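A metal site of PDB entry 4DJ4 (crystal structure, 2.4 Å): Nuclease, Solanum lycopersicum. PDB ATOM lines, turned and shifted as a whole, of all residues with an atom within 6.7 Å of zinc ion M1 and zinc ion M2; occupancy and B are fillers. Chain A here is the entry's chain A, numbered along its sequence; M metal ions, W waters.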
ATOM      1  N   TRP A   1       0.184  15.793 -21.706  1.00  0.00           N
ATOM      2  CA  TRP A   1      -0.760  16.811 -21.155  1.00  0.00           C
ATOM      3  C   TRP A   1      -0.332  18.169 -21.618  1.00  0.00           C
ATOM      4  O   TRP A   1       0.874  18.422 -21.860  1.00  0.00           O
ATOM      5  CB  TRP A   1      -0.760  16.850 -19.617  1.00  0.00           C
ATOM      6  CG  TRP A   1      -1.142  15.592 -18.898  1.00  0.00           C
ATOM      7  CD1 TRP A   1      -0.308  14.750 -18.182  1.00  0.00           C
ATOM      8  CD2 TRP A   1      -2.483  15.002 -18.736  1.00  0.00           C
ATOM      9  NE1 TRP A   1      -1.004  13.706 -17.638  1.00  0.00           N
ATOM     10  CE2 TRP A   1      -2.307  13.799 -17.933  1.00  0.00           C
ATOM     11  CE3 TRP A   1      -3.759  15.334 -19.168  1.00  0.00           C
ATOM     12  CZ2 TRP A   1      -3.382  12.992 -17.579  1.00  0.00           C
ATOM     13  CZ3 TRP A   1      -4.825  14.516 -18.815  1.00  0.00           C
ATOM     14  CH2 TRP A   1      -4.650  13.368 -18.042  1.00  0.00           C
ATOM     15  N   SER A   2      -1.310  19.086 -21.676  1.00  0.00           N
ATOM     16  CA  SER A   2      -0.987  20.503 -21.735  1.00  0.00           C
ATOM     17  C   SER A   2      -0.503  20.944 -20.320  1.00  0.00           C
ATOM     18  O   SER A   2      -0.372  20.126 -19.431  1.00  0.00           O
ATOM     19  CB  SER A   2      -2.191  21.322 -22.195  1.00  0.00           C
ATOM     20  OG  SER A   2      -2.627  20.935 -23.505  1.00  0.00           O
ATOM     21  N   LYS A   3      -0.237  22.231 -20.152  1.00  0.00           N
ATOM     22  CA  LYS A   3       0.366  22.804 -18.973  1.00  0.00           C
ATOM     23  C   LYS A   3      -0.229  22.272 -17.645  1.00  0.00           C
ATOM     24  O   LYS A   3       0.491  21.793 -16.776  1.00  0.00           O
ATOM     25  CB  LYS A   3       0.197  24.321 -19.072  1.00  0.00           C
ATOM     26  CG  LYS A   3       1.023  25.187 -18.141  1.00  0.00           C
ATOM     27  CD  LYS A   3       0.358  26.554 -17.959  1.00  0.00           C
ATOM     28  CE  LYS A   3       0.086  27.280 -19.288  1.00  0.00           C
ATOM     29  NZ  LYS A   3      -1.191  28.076 -19.268  1.00  0.00           N
ATOM     30  N   GLY A   5      -2.114  19.643 -16.718  1.00  0.00           N
ATOM     31  CA  GLY A   5      -1.948  18.257 -16.330  1.00  0.00           C
ATOM     32  C   GLY A   5      -0.566  18.020 -15.765  1.00  0.00           C
ATOM     33  O   GLY A   5      -0.410  17.286 -14.790  1.00  0.00           O
ATOM     34  N   HIS A   6       0.440  18.656 -16.379  1.00  0.00           N
ATOM     35  CA  HIS A   6       1.794  18.555 -15.866  1.00  0.00           C
ATOM     36  C   HIS A   6       1.974  19.226 -14.527  1.00  0.00           C
ATOM     37  O   HIS A   6       2.571  18.631 -13.625  1.00  0.00           O
ATOM     38  CB  HIS A   6       2.825  19.018 -16.886  1.00  0.00           C
ATOM     39  CG  HIS A   6       2.934  18.096 -18.047  1.00  0.00           C
ATOM     40  ND1 HIS A   6       3.421  16.848 -17.926  1.00  0.00           N
ATOM     41  CD2 HIS A   6       2.522  18.232 -19.386  1.00  0.00           C
ATOM     42  CE1 HIS A   6       3.331  16.225 -19.120  1.00  0.00           C
ATOM     43  NE2 HIS A   6       2.817  17.088 -20.013  1.00  0.00           N
ATOM     44  N   VAL A  42       6.609  21.554 -17.672  1.00  0.00           N
ATOM     45  CA  VAL A  42       6.176  21.643 -19.061  1.00  0.00           C
ATOM     46  C   VAL A  42       7.372  21.963 -19.985  1.00  0.00           C
ATOM     47  O   VAL A  42       7.232  21.967 -21.232  1.00  0.00           O
ATOM     48  CB  VAL A  42       4.985  22.652 -19.172  1.00  0.00           C
ATOM     49  CG1 VAL A  42       5.440  24.096 -19.117  1.00  0.00           C
ATOM     50  CG2 VAL A  42       4.150  22.374 -20.426  1.00  0.00           C
ATOM     51  N   PRO A  44       9.958  20.343 -21.067  1.00  0.00           N
ATOM     52  CA  PRO A  44      10.261  19.520 -22.259  1.00  0.00           C
ATOM     53  C   PRO A  44       9.378  19.758 -23.498  1.00  0.00           C
ATOM     54  O   PRO A  44       9.804  19.468 -24.604  1.00  0.00           O
ATOM     55  CB  PRO A  44      10.077  18.077 -21.744  1.00  0.00           C
ATOM     56  CG  PRO A  44      10.349  18.179 -20.279  1.00  0.00           C
ATOM     57  CD  PRO A  44       9.793  19.517 -19.852  1.00  0.00           C
ATOM     58  N   ASP A  45       8.148  20.261 -23.314  1.00  0.00           N
ATOM     59  CA  ASP A  45       7.264  20.525 -24.461  1.00  0.00           C
ATOM     60  C   ASP A  45       7.744  21.735 -25.289  1.00  0.00           C
ATOM     61  O   ASP A  45       7.425  21.837 -26.473  1.00  0.00           O
ATOM     62  CB  ASP A  45       5.809  20.778 -24.023  1.00  0.00           C
ATOM     63  CG  ASP A  45       4.999  19.490 -23.895  1.00  0.00           C
ATOM     64  OD1 ASP A  45       5.454  18.415 -24.329  1.00  0.00           O
ATOM     65  OD2 ASP A  45       3.888  19.557 -23.338  1.00  0.00           O
ATOM     66  N   ARG A  48      11.580  20.507 -26.963  1.00  0.00           N
ATOM     67  CA  ARG A  48      11.605  19.416 -27.967  1.00  0.00           C
ATOM     68  C   ARG A  48      11.782  19.945 -29.429  1.00  0.00           C
ATOM     69  O   ARG A  48      12.206  19.194 -30.310  1.00  0.00           O
ATOM     70  CB  ARG A  48      10.352  18.533 -27.865  1.00  0.00           C
ATOM     71  CG  ARG A  48       9.060  19.201 -28.298  1.00  0.00           C
ATOM     72  CD  ARG A  48       7.864  18.274 -28.122  1.00  0.00           C
ATOM     73  NE  ARG A  48       6.618  19.041 -28.013  1.00  0.00           N
ATOM     74  CZ  ARG A  48       5.702  19.199 -28.966  1.00  0.00           C
ATOM     75  NH1 ARG A  48       5.857  18.640 -30.182  1.00  0.00           N
ATOM     76  NH2 ARG A  48       4.620  19.935 -28.712  1.00  0.00           N
ATOM     77  N   LEU A  59       9.845  10.894 -27.533  1.00  0.00           N
ATOM     78  CA  LEU A  59       9.776  10.436 -26.136  1.00  0.00           C
ATOM     79  C   LEU A  59       8.488  10.859 -25.384  1.00  0.00           C
ATOM     80  O   LEU A  59       8.324  10.537 -24.199  1.00  0.00           O
ATOM     81  CB  LEU A  59      11.020  10.898 -25.373  1.00  0.00           C
ATOM     82  CG  LEU A  59      12.387  10.448 -25.945  1.00  0.00           C
ATOM     83  CD1 LEU A  59      13.473  10.735 -24.918  1.00  0.00           C
ATOM     84  CD2 LEU A  59      12.461   8.972 -26.372  1.00  0.00           C
ATOM     85  N   HIS A  60       7.592  11.569 -26.072  1.00  0.00           N
ATOM     86  CA  HIS A  60       6.384  12.127 -25.438  1.00  0.00           C
ATOM     87  C   HIS A  60       5.210  11.190 -25.543  1.00  0.00           C
ATOM     88  O   HIS A  60       4.208  11.363 -24.843  1.00  0.00           O
ATOM     89  CB  HIS A  60       6.045  13.500 -26.055  1.00  0.00           C
ATOM     90  CG  HIS A  60       6.973  14.609 -25.614  1.00  0.00           C
ATOM     91  ND1 HIS A  60       6.622  15.527 -24.673  1.00  0.00           N
ATOM     92  CD2 HIS A  60       8.277  14.904 -25.976  1.00  0.00           C
ATOM     93  CE1 HIS A  60       7.657  16.373 -24.459  1.00  0.00           C
ATOM     94  NE2 HIS A  60       8.678  15.990 -25.240  1.00  0.00           N
ATOM     95  N   PHE A  61       5.323  10.160 -26.382  1.00  0.00           N
ATOM     96  CA  PHE A  61       4.163   9.355 -26.721  1.00  0.00           C
ATOM     97  C   PHE A  61       4.552   7.961 -27.152  1.00  0.00           C
ATOM     98  O   PHE A  61       5.732   7.649 -27.316  1.00  0.00           O
ATOM     99  CB  PHE A  61       3.356  10.034 -27.845  1.00  0.00           C
ATOM    100  CG  PHE A  61       4.111  10.158 -29.144  1.00  0.00           C
ATOM    101  CD1 PHE A  61       4.308   9.050 -29.978  1.00  0.00           C
ATOM    102  CD2 PHE A  61       4.646  11.386 -29.537  1.00  0.00           C
ATOM    103  CE1 PHE A  61       5.026   9.154 -31.178  1.00  0.00           C
ATOM    104  CE2 PHE A  61       5.364  11.500 -30.738  1.00  0.00           C
ATOM    105  CZ  PHE A  61       5.545  10.386 -31.556  1.00  0.00           C
ATOM    106  N   HIS A 122       8.041  15.111 -16.612  1.00  0.00           N
ATOM    107  CA  HIS A 122       7.156  15.370 -17.726  1.00  0.00           C
ATOM    108  C   HIS A 122       6.627  14.084 -18.330  1.00  0.00           C
ATOM    109  O   HIS A 122       5.403  13.940 -18.531  1.00  0.00           O
ATOM    110  CB  HIS A 122       7.879  16.209 -18.799  1.00  0.00           C
ATOM    111  CG  HIS A 122       6.970  16.631 -19.929  1.00  0.00           C
ATOM    112  ND1 HIS A 122       6.283  17.790 -19.901  1.00  0.00           N
ATOM    113  CD2 HIS A 122       6.636  15.999 -21.130  1.00  0.00           C
ATOM    114  CE1 HIS A 122       5.549  17.891 -21.029  1.00  0.00           C
ATOM    115  NE2 HIS A 122       5.773  16.794 -21.778  1.00  0.00           N
ATOM    116  N   PHE A 123       7.538  13.156 -18.609  1.00  0.00           N
ATOM    117  CA  PHE A 123       7.200  11.936 -19.313  1.00  0.00           C
ATOM    118  C   PHE A 123       6.395  10.991 -18.432  1.00  0.00           C
ATOM    119  O   PHE A 123       5.633  10.188 -18.959  1.00  0.00           O
ATOM    120  CB  PHE A 123       8.443  11.236 -19.865  1.00  0.00           C
ATOM    121  CG  PHE A 123       9.146  11.997 -20.931  1.00  0.00           C
ATOM    122  CD1 PHE A 123       8.435  12.613 -21.949  1.00  0.00           C
ATOM    123  CD2 PHE A 123      10.537  12.056 -20.949  1.00  0.00           C
ATOM    124  CE1 PHE A 123       9.075  13.328 -22.957  1.00  0.00           C
ATOM    125  CE2 PHE A 123      11.184  12.784 -21.940  1.00  0.00           C
ATOM    126  CZ  PHE A 123      10.454  13.413 -22.954  1.00  0.00           C
ATOM    127  N   GLY A 125       3.996  12.119 -16.610  1.00  0.00           N
ATOM    128  CA  GLY A 125       2.672  12.650 -16.908  1.00  0.00           C
ATOM    129  C   GLY A 125       2.157  12.181 -18.267  1.00  0.00           C
ATOM    130  O   GLY A 125       1.034  11.677 -18.374  1.00  0.00           O
ATOM    131  N   ASP A 126       2.992  12.314 -19.295  1.00  0.00           N
ATOM    132  CA  ASP A 126       2.540  11.982 -20.651  1.00  0.00           C
ATOM    133  C   ASP A 126       2.108  10.552 -20.852  1.00  0.00           C
ATOM    134  O   ASP A 126       1.124  10.316 -21.517  1.00  0.00           O
ATOM    135  CB  ASP A 126       3.614  12.292 -21.705  1.00  0.00           C
ATOM    136  CG  ASP A 126       3.631  13.740 -22.106  1.00  0.00           C
ATOM    137  OD1 ASP A 126       2.712  14.516 -21.708  1.00  0.00           O
ATOM    138  OD2 ASP A 126       4.595  14.095 -22.836  1.00  0.00           O
ATOM    139  N   GLN A 129      -1.398  10.034 -19.784  1.00  0.00           N
ATOM    140  CA  GLN A 129      -2.425  10.635 -20.649  1.00  0.00           C
ATOM    141  C   GLN A 129      -2.761   9.577 -21.716  1.00  0.00           C
ATOM    142  O   GLN A 129      -1.943   9.317 -22.609  1.00  0.00           O
ATOM    143  CB  GLN A 129      -1.872  11.919 -21.299  1.00  0.00           C
ATOM    144  CG  GLN A 129      -2.891  12.985 -21.641  1.00  0.00           C
ATOM    145  CD  GLN A 129      -3.798  12.616 -22.807  1.00  0.00           C
ATOM    146  OE1 GLN A 129      -4.524  11.605 -22.745  1.00  0.00           O
ATOM    147  NE2 GLN A 129      -3.805  13.465 -23.866  1.00  0.00           N
ATOM    148  N   HIS A 132      -1.839   9.860 -25.340  1.00  0.00           N
ATOM    149  CA  HIS A 132      -0.408   9.816 -25.641  1.00  0.00           C
ATOM    150  C   HIS A 132       0.058   8.434 -25.959  1.00  0.00           C
ATOM    151  O   HIS A 132       1.218   8.230 -26.280  1.00  0.00           O
ATOM    152  CB  HIS A 132       0.449  10.400 -24.500  1.00  0.00           C
ATOM    153  CG  HIS A 132       0.729  11.865 -24.657  1.00  0.00           C
ATOM    154  ND1 HIS A 132       1.965  12.355 -24.805  1.00  0.00           N
ATOM    155  CD2 HIS A 132      -0.130  12.954 -24.714  1.00  0.00           C
ATOM    156  CE1 HIS A 132       1.897  13.678 -24.971  1.00  0.00           C
ATOM    157  NE2 HIS A 132       0.611  14.044 -24.908  1.00  0.00           N
ATOM    158  N   ASP A 160      -5.612  16.222 -23.452  1.00  0.00           N
ATOM    159  CA  ASP A 160      -4.513  17.047 -22.970  1.00  0.00           C
ATOM    160  C   ASP A 160      -4.980  18.261 -22.141  1.00  0.00           C
ATOM    161  O   ASP A 160      -4.226  18.713 -21.288  1.00  0.00           O
ATOM    162  CB  ASP A 160      -3.678  17.623 -24.146  1.00  0.00           C
ATOM    163  CG  ASP A 160      -2.485  16.780 -24.545  1.00  0.00           C
ATOM    164  OD1 ASP A 160      -2.127  15.807 -23.843  1.00  0.00           O
ATOM    165  OD2 ASP A 160      -1.879  17.097 -25.582  1.00  0.00           O
HETATM  166 ZN    ZN M   1       2.027  16.485 -21.711  1.00  0.00          ZN
HETATM  167 ZN    ZN M   2       4.825  16.174 -23.540  1.00  0.00          ZN
HETATM  168 ZN    ZN M   3      -0.405  15.779 -25.864  1.00  0.00          ZN
HETATM  169  O   HOH W   1       4.065  16.254 -25.873  1.00  0.00           O
HETATM  170  O   HOH W   2       0.792  17.262 -24.576  1.00  0.00           O
HETATM  171  O   HOH W   3       3.043  16.953 -23.477  1.00  0.00           O
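N of Trp 1 sits close to OD1 of Asp 160.
The guanidinium group (NE) of Arg 48 sits at hydrogen-bond distance from the backbone carbonyl oxygen (O) of Asp 45 (3.3 Å).
The backbone carbonyl oxygen (O) of His 60 is in hydrogen-bond range of a ring nitrogen (ND1) of His 132 (2.5 Å).
The indole nitrogen of Trp 1 lies within hydrogen-bond range of the backbone carbonyl oxygen of Gly 125 (3.0 Å).
Within 4 Å of zinc ion M1: Trp 1, His 6, Asp 45, His 122 and Asp 126.
Zinc ion M2 is bound by water W3 (1.9 Å).
Zinc ion M2 is bound by a ring nitrogen (NE2) of His 122 (2.1 Å).
OD2 of Asp 126 is bound to zinc ion M2, at 2.2 Å.
ND1 of His 60 binds zinc ion M2, 2.2 Å away.
Zinc ion M2 is bound by water W1.
OD1 of Asp 45 is bound to zinc ion M2, 2.5 Å away.
Zinc ion M2 has six donor atoms within binding distance.
Zinc ion M1 is bound by NE2 of His 6, N of Trp 1, OD1 of Asp 126, water W3 and O of Trp 1.
Zinc ion M1 has five donor atoms within binding distance.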
